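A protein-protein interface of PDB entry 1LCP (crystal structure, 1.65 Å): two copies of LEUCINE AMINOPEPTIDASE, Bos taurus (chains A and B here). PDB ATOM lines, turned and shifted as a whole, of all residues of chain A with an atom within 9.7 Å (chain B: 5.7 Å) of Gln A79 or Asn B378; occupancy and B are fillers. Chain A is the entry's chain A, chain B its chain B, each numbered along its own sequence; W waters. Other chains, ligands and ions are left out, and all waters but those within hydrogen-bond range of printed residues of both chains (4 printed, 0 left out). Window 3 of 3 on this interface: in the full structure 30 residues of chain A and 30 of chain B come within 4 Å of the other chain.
NE2 of Gln A79 sits at hydrogen-bond distance from O of Asn B378 (2.9 Å).
The backbone carbonyl oxygen (O) of Arg B399 is in hydrogen-bond range of the indole nitrogen (NE1) of Trp A398 (2.8 Å).
N of Glu A80 is in hydrogen-bond range of OD1 of Asp A77 (3.4 Å).
The side-chain carboxylate (OE1) of Glu A80 lies within salt-bridge range of the guanidinium group (NH1) of Arg A396, 2.8 Å away.
NH2 of Arg B399 sits at hydrogen-bond distance from O of Thr B377 (3.1 Å).
The side-chain amide nitrogen (ND2) of Asn B378 lies within hydrogen-bond range of the backbone carbonyl oxygen (O) of His B442 (2.8 Å).
The side-chain amide oxygen (OD1) of Asn B378 sits close to the backbone carbonyl oxygen (O) of Pro B443 (3.3 Å).
The side-chain hydroxyl of Ser B380 lies within hydrogen-bond range of the guanidinium group of Arg B399.
Gln A79 touches Leu B402 (O to O, 3.99 Å).
Gln A79 touches Phe B403 (O to CE1, 3.8 Å).
Phe B403 touches Glu A80.
Arg A396 touches Phe B403 (CZ to CD2, 3.4 Å).
Trp A398 touches Phe B403.
Printed residues of chain B within 4 Å of Gln A79: Asn B378 (2.9 Å), Leu B402 (3.99 Å) and Phe B403 (3.8 Å).
Asn B378 touches one residue of chain A.
No residue of chain A comes within 4 Å of Thr B377.
Of the printed residues of chain B, Glu A80 touches Phe B403.
Printed residues of chain A within 4 Å of Arg B399: Trp A398.
Of the printed residues of chain B, Arg A396 touches Phe B403 (3.4 Å).
Printed residues of chain B within 4 Å of Trp A398: Arg B399 and Phe B403.
Of the printed residues of chain A, Leu B402 touches Gln A79 (3.99 Å).
Ile A76 touches none of the printed residues of chain B.
His B442 touches none of the printed residues of chain A.
The nearest residue of chain A that does not touch Asn B378 is Glu A78 (6.8 Å).
The nearest printed residue of chain A that does not touch Leu B402 is Glu A80 (4.4 Å).
Of the 14 printed residues of chain B, 4 touch a printed residue of chain A.
Hydrophobic or aromatic side chains of chain A that line the printed part of chain B: Trp A398.
Among the printed residues, no Asp or Glu carboxylate lies within 4 Å of a Lys or Arg side-chain nitrogen of the other chain.
No position is printed for both chains.
Of the 7 pairs that touch across the chains among the printed residues, none has its exchanged pair printed and touching as well.
Water W4 bridges the side-chain carboxylate of Glu A80 (2.7 Å) and the backbone carbonyl oxygen of Leu B402 (3.1 Å).
Water W3 lies within hydrogen-bond range of OE1 of Gln A79 (2.9 Å) and O of Leu B402 (3.2 Å).
Water W1 lies within hydrogen-bond range of the guanidinium group (NH2) of Arg B399 (2.9 Å), the side-chain hydroxyl (OG) of Ser B380 (3.2 Å), the backbone carbonyl oxygen (O) of Asn B378 (3.5 Å) and the side-chain amide oxygen (OE1) of Gln A79 (3.5 Å).
Water W2 lies within hydrogen-bond range of O of Arg B399 (3.0 Å) and NE1 of Trp A398 (3.1 Å).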
ATOM      1  N   GLY A  75      -4.039 -15.279   2.189  1.00  0.00           N
ATOM      2  CA  GLY A  75      -3.362 -16.507   2.563  1.00  0.00           C
ATOM      3  C   GLY A  75      -3.079 -17.355   1.348  1.00  0.00           C
ATOM      4  O   GLY A  75      -2.681 -16.840   0.294  1.00  0.00           O
ATOM      5  N   ILE A  76      -3.243 -18.664   1.499  1.00  0.00           N
ATOM      6  CA  ILE A  76      -3.022 -19.590   0.400  1.00  0.00           C
ATOM      7  C   ILE A  76      -4.141 -19.412  -0.621  1.00  0.00           C
ATOM      8  O   ILE A  76      -5.325 -19.433  -0.269  1.00  0.00           O
ATOM      9  CB  ILE A  76      -2.972 -21.059   0.901  1.00  0.00           C
ATOM     10  CG1 ILE A  76      -1.702 -21.274   1.745  1.00  0.00           C
ATOM     11  CG2 ILE A  76      -2.995 -22.029  -0.273  1.00  0.00           C
ATOM     12  CD1 ILE A  76      -1.548 -22.683   2.334  1.00  0.00           C
ATOM     13  N   ASP A  77      -3.757 -19.137  -1.866  1.00  0.00           N
ATOM     14  CA  ASP A  77      -4.701 -18.956  -2.959  1.00  0.00           C
ATOM     15  C   ASP A  77      -4.850 -20.337  -3.606  1.00  0.00           C
ATOM     16  O   ASP A  77      -3.930 -20.825  -4.276  1.00  0.00           O
ATOM     17  CB  ASP A  77      -4.138 -17.932  -3.955  1.00  0.00           C
ATOM     18  CG  ASP A  77      -5.113 -17.581  -5.073  1.00  0.00           C
ATOM     19  OD1 ASP A  77      -5.952 -18.423  -5.465  1.00  0.00           O
ATOM     20  OD2 ASP A  77      -5.027 -16.454  -5.599  1.00  0.00           O
ATOM     21  N   GLU A  78      -6.004 -20.968  -3.400  1.00  0.00           N
ATOM     22  CA  GLU A  78      -6.259 -22.297  -3.943  1.00  0.00           C
ATOM     23  C   GLU A  78      -6.191 -22.366  -5.472  1.00  0.00           C
ATOM     24  O   GLU A  78      -5.970 -23.438  -6.025  1.00  0.00           O
ATOM     25  CB  GLU A  78      -7.607 -22.847  -3.455  1.00  0.00           C
ATOM     26  CG  GLU A  78      -7.943 -22.588  -1.980  1.00  0.00           C
ATOM     27  CD  GLU A  78      -6.836 -22.974  -0.999  1.00  0.00           C
ATOM     28  OE1 GLU A  78      -6.233 -24.070  -1.153  1.00  0.00           O
ATOM     29  OE2 GLU A  78      -6.590 -22.183  -0.047  1.00  0.00           O
ATOM     30  N   GLN A  79      -6.379 -21.242  -6.157  1.00  0.00           N
ATOM     31  CA  GLN A  79      -6.313 -21.232  -7.619  1.00  0.00           C
ATOM     32  C   GLN A  79      -4.882 -21.126  -8.164  1.00  0.00           C
ATOM     33  O   GLN A  79      -4.558 -21.700  -9.205  1.00  0.00           O
ATOM     34  CB  GLN A  79      -7.146 -20.074  -8.179  1.00  0.00           C
ATOM     35  CG  GLN A  79      -8.630 -20.097  -7.793  1.00  0.00           C
ATOM     36  CD  GLN A  79      -9.375 -21.282  -8.377  1.00  0.00           C
ATOM     37  OE1 GLN A  79      -9.014 -21.807  -9.437  1.00  0.00           O
ATOM     38  NE2 GLN A  79     -10.446 -21.685  -7.714  1.00  0.00           N
ATOM     39  N   GLU A  80      -4.028 -20.402  -7.450  1.00  0.00           N
ATOM     40  CA  GLU A  80      -2.648 -20.179  -7.879  1.00  0.00           C
ATOM     41  C   GLU A  80      -1.612 -21.126  -7.252  1.00  0.00           C
ATOM     42  O   GLU A  80      -0.442 -21.106  -7.629  1.00  0.00           O
ATOM     43  CB  GLU A  80      -2.246 -18.722  -7.611  1.00  0.00           C
ATOM     44  CG  GLU A  80      -3.064 -17.653  -8.354  1.00  0.00           C
ATOM     45  CD  GLU A  80      -2.788 -17.599  -9.853  1.00  0.00           C
ATOM     46  OE1 GLU A  80      -1.739 -18.110 -10.297  1.00  0.00           O
ATOM     47  OE2 GLU A  80      -3.620 -17.033 -10.599  1.00  0.00           O
ATOM     48  N   ASN A  81      -2.034 -21.925  -6.278  1.00  0.00           N
ATOM     49  CA  ASN A  81      -1.138 -22.865  -5.608  1.00  0.00           C
ATOM     50  C   ASN A  81       0.071 -22.209  -4.938  1.00  0.00           C
ATOM     51  O   ASN A  81       1.208 -22.680  -5.080  1.00  0.00           O
ATOM     52  CB  ASN A  81      -0.664 -23.977  -6.567  1.00  0.00           C
ATOM     53  CG  ASN A  81      -1.810 -24.842  -7.116  1.00  0.00           C
ATOM     54  OD1 ASN A  81      -1.662 -25.475  -8.166  1.00  0.00           O
ATOM     55  ND2 ASN A  81      -2.943 -24.866  -6.424  1.00  0.00           N
ATOM     56  N   TRP A  82      -0.168 -21.109  -4.224  1.00  0.00           N
ATOM     57  CA  TRP A  82       0.894 -20.423  -3.477  1.00  0.00           C
ATOM     58  C   TRP A  82       0.303 -19.568  -2.367  1.00  0.00           C
ATOM     59  O   TRP A  82      -0.917 -19.350  -2.321  1.00  0.00           O
ATOM     60  CB  TRP A  82       1.808 -19.555  -4.381  1.00  0.00           C
ATOM     61  CG  TRP A  82       1.185 -18.377  -5.143  1.00  0.00           C
ATOM     62  CD1 TRP A  82      -0.011 -17.740  -4.890  1.00  0.00           C
ATOM     63  CD2 TRP A  82       1.767 -17.688  -6.272  1.00  0.00           C
ATOM     64  NE1 TRP A  82      -0.194 -16.708  -5.792  1.00  0.00           N
ATOM     65  CE2 TRP A  82       0.878 -16.658  -6.646  1.00  0.00           C
ATOM     66  CE3 TRP A  82       2.961 -17.852  -6.999  1.00  0.00           C
ATOM     67  CZ2 TRP A  82       1.140 -15.788  -7.720  1.00  0.00           C
ATOM     68  CZ3 TRP A  82       3.222 -16.984  -8.069  1.00  0.00           C
ATOM     69  CH2 TRP A  82       2.312 -15.969  -8.415  1.00  0.00           C
ATOM     70  N   HIS A  83       1.159 -19.140  -1.446  1.00  0.00           N
ATOM     71  CA  HIS A  83       0.734 -18.256  -0.370  1.00  0.00           C
ATOM     72  C   HIS A  83       0.836 -16.851  -0.969  1.00  0.00           C
ATOM     73  O   HIS A  83       1.934 -16.324  -1.187  1.00  0.00           O
ATOM     74  CB  HIS A  83       1.647 -18.387   0.856  1.00  0.00           C
ATOM     75  CG  HIS A  83       1.123 -17.667   2.062  1.00  0.00           C
ATOM     76  ND1 HIS A  83       1.004 -16.294   2.122  1.00  0.00           N
ATOM     77  CD2 HIS A  83       0.673 -18.133   3.254  1.00  0.00           C
ATOM     78  CE1 HIS A  83       0.508 -15.945   3.292  1.00  0.00           C
ATOM     79  NE2 HIS A  83       0.296 -17.040   3.996  1.00  0.00           N
ATOM     80  N   GLU A  84      -0.319 -16.270  -1.263  1.00  0.00           N
ATOM     81  CA  GLU A  84      -0.401 -14.952  -1.888  1.00  0.00           C
ATOM     82  C   GLU A  84       0.196 -13.828  -1.044  1.00  0.00           C
ATOM     83  O   GLU A  84       0.842 -12.933  -1.583  1.00  0.00           O
ATOM     84  CB  GLU A  84      -1.858 -14.631  -2.267  1.00  0.00           C
ATOM     85  CG  GLU A  84      -2.060 -13.245  -2.883  1.00  0.00           C
ATOM     86  CD  GLU A  84      -3.527 -12.912  -3.161  1.00  0.00           C
ATOM     87  OE1 GLU A  84      -4.429 -13.581  -2.610  1.00  0.00           O
ATOM     88  OE2 GLU A  84      -3.781 -11.974  -3.946  1.00  0.00           O
ATOM     89  N   PHE A 387       5.259 -30.279  -3.890  1.00  0.00           N
ATOM     90  CA  PHE A 387       4.138 -29.376  -4.140  1.00  0.00           C
ATOM     91  C   PHE A 387       3.888 -28.480  -2.922  1.00  0.00           C
ATOM     92  O   PHE A 387       3.793 -27.253  -3.044  1.00  0.00           O
ATOM     93  CB  PHE A 387       2.882 -30.199  -4.480  1.00  0.00           C
ATOM     94  CG  PHE A 387       1.638 -29.372  -4.691  1.00  0.00           C
ATOM     95  CD1 PHE A 387       1.560 -28.448  -5.732  1.00  0.00           C
ATOM     96  CD2 PHE A 387       0.545 -29.523  -3.846  1.00  0.00           C
ATOM     97  CE1 PHE A 387       0.417 -27.684  -5.931  1.00  0.00           C
ATOM     98  CE2 PHE A 387      -0.616 -28.753  -4.040  1.00  0.00           C
ATOM     99  CZ  PHE A 387      -0.672 -27.835  -5.086  1.00  0.00           C
ATOM    100  N   ILE A 391       4.309 -24.149  -2.433  1.00  0.00           N
ATOM    101  CA  ILE A 391       3.235 -23.237  -2.033  1.00  0.00           C
ATOM    102  C   ILE A 391       3.830 -22.172  -1.099  1.00  0.00           C
ATOM    103  O   ILE A 391       3.539 -20.970  -1.221  1.00  0.00           O
ATOM    104  CB  ILE A 391       2.084 -24.007  -1.317  1.00  0.00           C
ATOM    105  CG1 ILE A 391       1.419 -24.973  -2.313  1.00  0.00           C
ATOM    106  CG2 ILE A 391       1.053 -23.017  -0.736  1.00  0.00           C
ATOM    107  CD1 ILE A 391       0.357 -25.861  -1.722  1.00  0.00           C
ATOM    108  N   ARG A 396       6.731 -22.207  -7.864  1.00  0.00           N
ATOM    109  CA  ARG A 396       5.873 -23.339  -8.210  1.00  0.00           C
ATOM    110  C   ARG A 396       6.352 -24.536  -9.034  1.00  0.00           C
ATOM    111  O   ARG A 396       7.227 -24.418  -9.892  1.00  0.00           O
ATOM    112  CB  ARG A 396       4.571 -22.795  -8.808  1.00  0.00           C
ATOM    113  CG  ARG A 396       3.909 -21.729  -7.924  1.00  0.00           C
ATOM    114  CD  ARG A 396       2.607 -21.194  -8.526  1.00  0.00           C
ATOM    115  NE  ARG A 396       2.843 -20.217  -9.591  1.00  0.00           N
ATOM    116  CZ  ARG A 396       1.908 -19.410 -10.082  1.00  0.00           C
ATOM    117  NH1 ARG A 396       0.658 -19.495  -9.646  1.00  0.00           N
ATOM    118  NH2 ARG A 396       2.217 -18.544 -11.035  1.00  0.00           N
ATOM    119  N   TRP A 398       4.757 -28.238 -11.111  1.00  0.00           N
ATOM    120  CA  TRP A 398       3.548 -28.775 -11.745  1.00  0.00           C
ATOM    121  C   TRP A 398       3.860 -30.183 -12.227  1.00  0.00           C
ATOM    122  O   TRP A 398       4.874 -30.404 -12.890  1.00  0.00           O
ATOM    123  CB  TRP A 398       3.117 -27.881 -12.919  1.00  0.00           C
ATOM    124  CG  TRP A 398       1.742 -28.205 -13.436  1.00  0.00           C
ATOM    125  CD1 TRP A 398       1.429 -29.056 -14.467  1.00  0.00           C
ATOM    126  CD2 TRP A 398       0.493 -27.737 -12.908  1.00  0.00           C
ATOM    127  NE1 TRP A 398       0.066 -29.151 -14.602  1.00  0.00           N
ATOM    128  CE2 TRP A 398      -0.536 -28.353 -13.657  1.00  0.00           C
ATOM    129  CE3 TRP A 398       0.141 -26.860 -11.870  1.00  0.00           C
ATOM    130  CZ2 TRP A 398      -1.897 -28.123 -13.403  1.00  0.00           C
ATOM    131  CZ3 TRP A 398      -1.218 -26.627 -11.615  1.00  0.00           C
ATOM    132  CH2 TRP A 398      -2.219 -27.262 -12.382  1.00  0.00           C
ATOM    133  N   PHE B 376      -7.684 -27.713 -18.244  1.00  0.00           N
ATOM    134  CA  PHE B 376      -7.488 -26.437 -17.539  1.00  0.00           C
ATOM    135  C   PHE B 376      -8.817 -26.149 -16.816  1.00  0.00           C
ATOM    136  O   PHE B 376      -9.865 -26.075 -17.466  1.00  0.00           O
ATOM    137  CB  PHE B 376      -7.202 -25.286 -18.524  1.00  0.00           C
ATOM    138  CG  PHE B 376      -5.878 -25.391 -19.247  1.00  0.00           C
ATOM    139  CD1 PHE B 376      -5.782 -26.062 -20.463  1.00  0.00           C
ATOM    140  CD2 PHE B 376      -4.737 -24.781 -18.730  1.00  0.00           C
ATOM    141  CE1 PHE B 376      -4.570 -26.124 -21.161  1.00  0.00           C
ATOM    142  CE2 PHE B 376      -3.526 -24.832 -19.417  1.00  0.00           C
ATOM    143  CZ  PHE B 376      -3.441 -25.507 -20.639  1.00  0.00           C
ATOM    144  N   THR B 377      -8.792 -25.978 -15.494  1.00  0.00           N
ATOM    145  CA  THR B 377     -10.033 -25.717 -14.756  1.00  0.00           C
ATOM    146  C   THR B 377      -9.856 -24.900 -13.471  1.00  0.00           C
ATOM    147  O   THR B 377      -8.829 -25.003 -12.801  1.00  0.00           O
ATOM    148  CB  THR B 377     -10.783 -27.056 -14.424  1.00  0.00           C
ATOM    149  OG1 THR B 377     -12.033 -26.780 -13.776  1.00  0.00           O
ATOM    150  CG2 THR B 377      -9.939 -27.978 -13.525  1.00  0.00           C
ATOM    151  N   ASN B 378     -10.866 -24.095 -13.132  1.00  0.00           N
ATOM    152  CA  ASN B 378     -10.839 -23.293 -11.901  1.00  0.00           C
ATOM    153  C   ASN B 378     -11.506 -24.047 -10.745  1.00  0.00           C
ATOM    154  O   ASN B 378     -11.691 -23.501  -9.653  1.00  0.00           O
ATOM    155  CB  ASN B 378     -11.517 -21.923 -12.114  1.00  0.00           C
ATOM    156  CG  ASN B 378     -12.986 -22.035 -12.539  1.00  0.00           C
ATOM    157  OD1 ASN B 378     -13.515 -23.139 -12.745  1.00  0.00           O
ATOM    158  ND2 ASN B 378     -13.651 -20.886 -12.665  1.00  0.00           N
ATOM    159  N   SER B 379     -11.811 -25.324 -10.970  1.00  0.00           N
ATOM    160  CA  SER B 379     -12.474 -26.152  -9.963  1.00  0.00           C
ATOM    161  C   SER B 379     -11.790 -27.506  -9.758  1.00  0.00           C
ATOM    162  O   SER B 379     -11.848 -28.386 -10.625  1.00  0.00           O
ATOM    163  CB  SER B 379     -13.946 -26.366 -10.361  1.00  0.00           C
ATOM    164  OG  SER B 379     -14.575 -27.357  -9.556  1.00  0.00           O
ATOM    165  N   SER B 380     -11.198 -27.705  -8.585  1.00  0.00           N
ATOM    166  CA  SER B 380     -10.534 -28.974  -8.293  1.00  0.00           C
ATOM    167  C   SER B 380     -11.560 -30.113  -8.187  1.00  0.00           C
ATOM    168  O   SER B 380     -11.247 -31.266  -8.478  1.00  0.00           O
ATOM    169  CB  SER B 380      -9.671 -28.850  -7.040  1.00  0.00           C
ATOM    170  OG  SER B 380      -8.541 -28.037  -7.314  1.00  0.00           O
ATOM    171  N   ARG B 399      -4.083 -32.674 -15.817  1.00  0.00           N
ATOM    172  CA  ARG B 399      -4.290 -31.251 -15.496  1.00  0.00           C
ATOM    173  C   ARG B 399      -3.153 -30.325 -15.928  1.00  0.00           C
ATOM    174  O   ARG B 399      -1.969 -30.694 -15.826  1.00  0.00           O
ATOM    175  CB  ARG B 399      -4.579 -31.059 -13.997  1.00  0.00           C
ATOM    176  CG  ARG B 399      -5.328 -29.758 -13.691  1.00  0.00           C
ATOM    177  CD  ARG B 399      -5.749 -29.641 -12.230  1.00  0.00           C
ATOM    178  NE  ARG B 399      -6.557 -28.437 -11.989  1.00  0.00           N
ATOM    179  CZ  ARG B 399      -7.101 -28.109 -10.815  1.00  0.00           C
ATOM    180  NH1 ARG B 399      -6.936 -28.887  -9.749  1.00  0.00           N
ATOM    181  NH2 ARG B 399      -7.819 -26.998 -10.712  1.00  0.00           N
ATOM    182  N   LEU B 402      -3.923 -23.012 -14.732  1.00  0.00           N
ATOM    183  CA  LEU B 402      -4.733 -21.848 -15.052  1.00  0.00           C
ATOM    184  C   LEU B 402      -4.252 -20.753 -14.072  1.00  0.00           C
ATOM    185  O   LEU B 402      -4.840 -20.547 -13.011  1.00  0.00           O
ATOM    186  CB  LEU B 402      -6.221 -22.173 -14.854  1.00  0.00           C
ATOM    187  CG  LEU B 402      -7.278 -21.321 -15.559  1.00  0.00           C
ATOM    188  CD1 LEU B 402      -7.109 -21.402 -17.072  1.00  0.00           C
ATOM    189  CD2 LEU B 402      -8.668 -21.811 -15.162  1.00  0.00           C
ATOM    190  N   PHE B 403      -3.149 -20.095 -14.425  1.00  0.00           N
ATOM    191  CA  PHE B 403      -2.522 -19.059 -13.589  1.00  0.00           C
ATOM    192  C   PHE B 403      -2.600 -17.641 -14.200  1.00  0.00           C
ATOM    193  O   PHE B 403      -2.471 -17.472 -15.422  1.00  0.00           O
ATOM    194  CB  PHE B 403      -1.016 -19.372 -13.401  1.00  0.00           C
ATOM    195  CG  PHE B 403      -0.700 -20.652 -12.637  1.00  0.00           C
ATOM    196  CD1 PHE B 403      -1.630 -21.272 -11.810  1.00  0.00           C
ATOM    197  CD2 PHE B 403       0.595 -21.189 -12.698  1.00  0.00           C
ATOM    198  CE1 PHE B 403      -1.278 -22.402 -11.051  1.00  0.00           C
ATOM    199  CE2 PHE B 403       0.959 -22.313 -11.941  1.00  0.00           C
ATOM    200  CZ  PHE B 403       0.022 -22.921 -11.115  1.00  0.00           C
ATOM    201  N   VAL B 440     -15.012 -16.015 -19.276  1.00  0.00           N
ATOM    202  CA  VAL B 440     -15.711 -16.900 -18.351  1.00  0.00           C
ATOM    203  C   VAL B 440     -15.736 -16.324 -16.930  1.00  0.00           C
ATOM    204  O   VAL B 440     -14.718 -15.866 -16.423  1.00  0.00           O
ATOM    205  CB  VAL B 440     -15.033 -18.306 -18.296  1.00  0.00           C
ATOM    206  CG1 VAL B 440     -15.689 -19.173 -17.214  1.00  0.00           C
ATOM    207  CG2 VAL B 440     -15.108 -19.002 -19.666  1.00  0.00           C
ATOM    208  N   HIS B 442     -17.892 -18.095 -14.569  1.00  0.00           N
ATOM    209  CA  HIS B 442     -18.475 -19.231 -13.855  1.00  0.00           C
ATOM    210  C   HIS B 442     -17.476 -19.924 -12.907  1.00  0.00           C
ATOM    211  O   HIS B 442     -16.320 -20.132 -13.271  1.00  0.00           O
ATOM    212  CB  HIS B 442     -18.982 -20.217 -14.914  1.00  0.00           C
ATOM    213  CG  HIS B 442     -19.876 -21.287 -14.375  1.00  0.00           C
ATOM    214  ND1 HIS B 442     -21.256 -21.193 -14.425  1.00  0.00           N
ATOM    215  CD2 HIS B 442     -19.601 -22.454 -13.762  1.00  0.00           C
ATOM    216  CE1 HIS B 442     -21.781 -22.262 -13.857  1.00  0.00           C
ATOM    217  NE2 HIS B 442     -20.796 -23.047 -13.441  1.00  0.00           N
ATOM    218  N   PRO B 443     -17.934 -20.366 -11.714  1.00  0.00           N
ATOM    219  CA  PRO B 443     -17.055 -21.032 -10.738  1.00  0.00           C
ATOM    220  C   PRO B 443     -16.655 -22.494 -11.030  1.00  0.00           C
ATOM    221  O   PRO B 443     -15.767 -23.038 -10.376  1.00  0.00           O
ATOM    222  CB  PRO B 443     -17.846 -20.921  -9.438  1.00  0.00           C
ATOM    223  CG  PRO B 443     -19.263 -21.019  -9.907  1.00  0.00           C
ATOM    224  CD  PRO B 443     -19.276 -20.140 -11.144  1.00  0.00           C
ATOM    225  N   LYS B 444     -17.310 -23.130 -11.995  1.00  0.00           N
ATOM    226  CA  LYS B 444     -17.012 -24.519 -12.354  1.00  0.00           C
ATOM    227  C   LYS B 444     -16.887 -24.668 -13.872  1.00  0.00           C
ATOM    228  O   LYS B 444     -17.811 -25.140 -14.554  1.00  0.00           O
ATOM    229  CB  LYS B 444     -18.081 -25.476 -11.795  1.00  0.00           C
ATOM    230  CG  LYS B 444     -18.057 -25.613 -10.278  1.00  0.00           C
ATOM    231  CD  LYS B 444     -19.066 -26.660  -9.805  1.00  0.00           C
ATOM    232  CE  LYS B 444     -18.908 -26.950  -8.319  1.00  0.00           C
ATOM    233  NZ  LYS B 444     -19.065 -25.726  -7.479  1.00  0.00           N
ATOM    234  N   TRP B 445     -15.746 -24.224 -14.388  1.00  0.00           N
ATOM    235  CA  TRP B 445     -15.456 -24.278 -15.818  1.00  0.00           C
ATOM    236  C   TRP B 445     -14.212 -25.124 -16.089  1.00  0.00           C
ATOM    237  O   TRP B 445     -13.229 -25.032 -15.355  1.00  0.00           O
ATOM    238  CB  TRP B 445     -15.222 -22.856 -16.348  1.00  0.00           C
ATOM    239  CG  TRP B 445     -14.601 -22.811 -17.719  1.00  0.00           C
ATOM    240  CD1 TRP B 445     -15.190 -23.192 -18.895  1.00  0.00           C
ATOM    241  CD2 TRP B 445     -13.289 -22.333 -18.059  1.00  0.00           C
ATOM    242  NE1 TRP B 445     -14.327 -22.974 -19.947  1.00  0.00           N
ATOM    243  CE2 TRP B 445     -13.154 -22.443 -19.466  1.00  0.00           C
ATOM    244  CE3 TRP B 445     -12.215 -21.809 -17.319  1.00  0.00           C
ATOM    245  CZ2 TRP B 445     -11.988 -22.055 -20.153  1.00  0.00           C
ATOM    246  CZ3 TRP B 445     -11.051 -21.422 -18.001  1.00  0.00           C
ATOM    247  CH2 TRP B 445     -10.953 -21.546 -19.407  1.00  0.00           C
ATOM    248  N   ALA B 446     -14.260 -25.933 -17.148  1.00  0.00           N
ATOM    249  CA  ALA B 446     -13.133 -26.771 -17.554  1.00  0.00           C
ATOM    250  C   ALA B 446     -12.947 -26.672 -19.070  1.00  0.00           C
ATOM    251  O   ALA B 446     -13.916 -26.714 -19.834  1.00  0.00           O
ATOM    252  CB  ALA B 446     -13.352 -28.234 -17.150  1.00  0.00           C
HETATM  253  O   HOH W   1      -8.834 -25.175  -8.679  1.00  0.00           O
HETATM  254  O   HOH W   2      -0.647 -31.928 -13.493  1.00  0.00           O
HETATM  255  O   HOH W   3      -6.764 -22.344 -11.132  1.00  0.00           O
HETATM  256  O   HOH W   4      -5.956 -18.033 -11.625  1.00  0.00           O
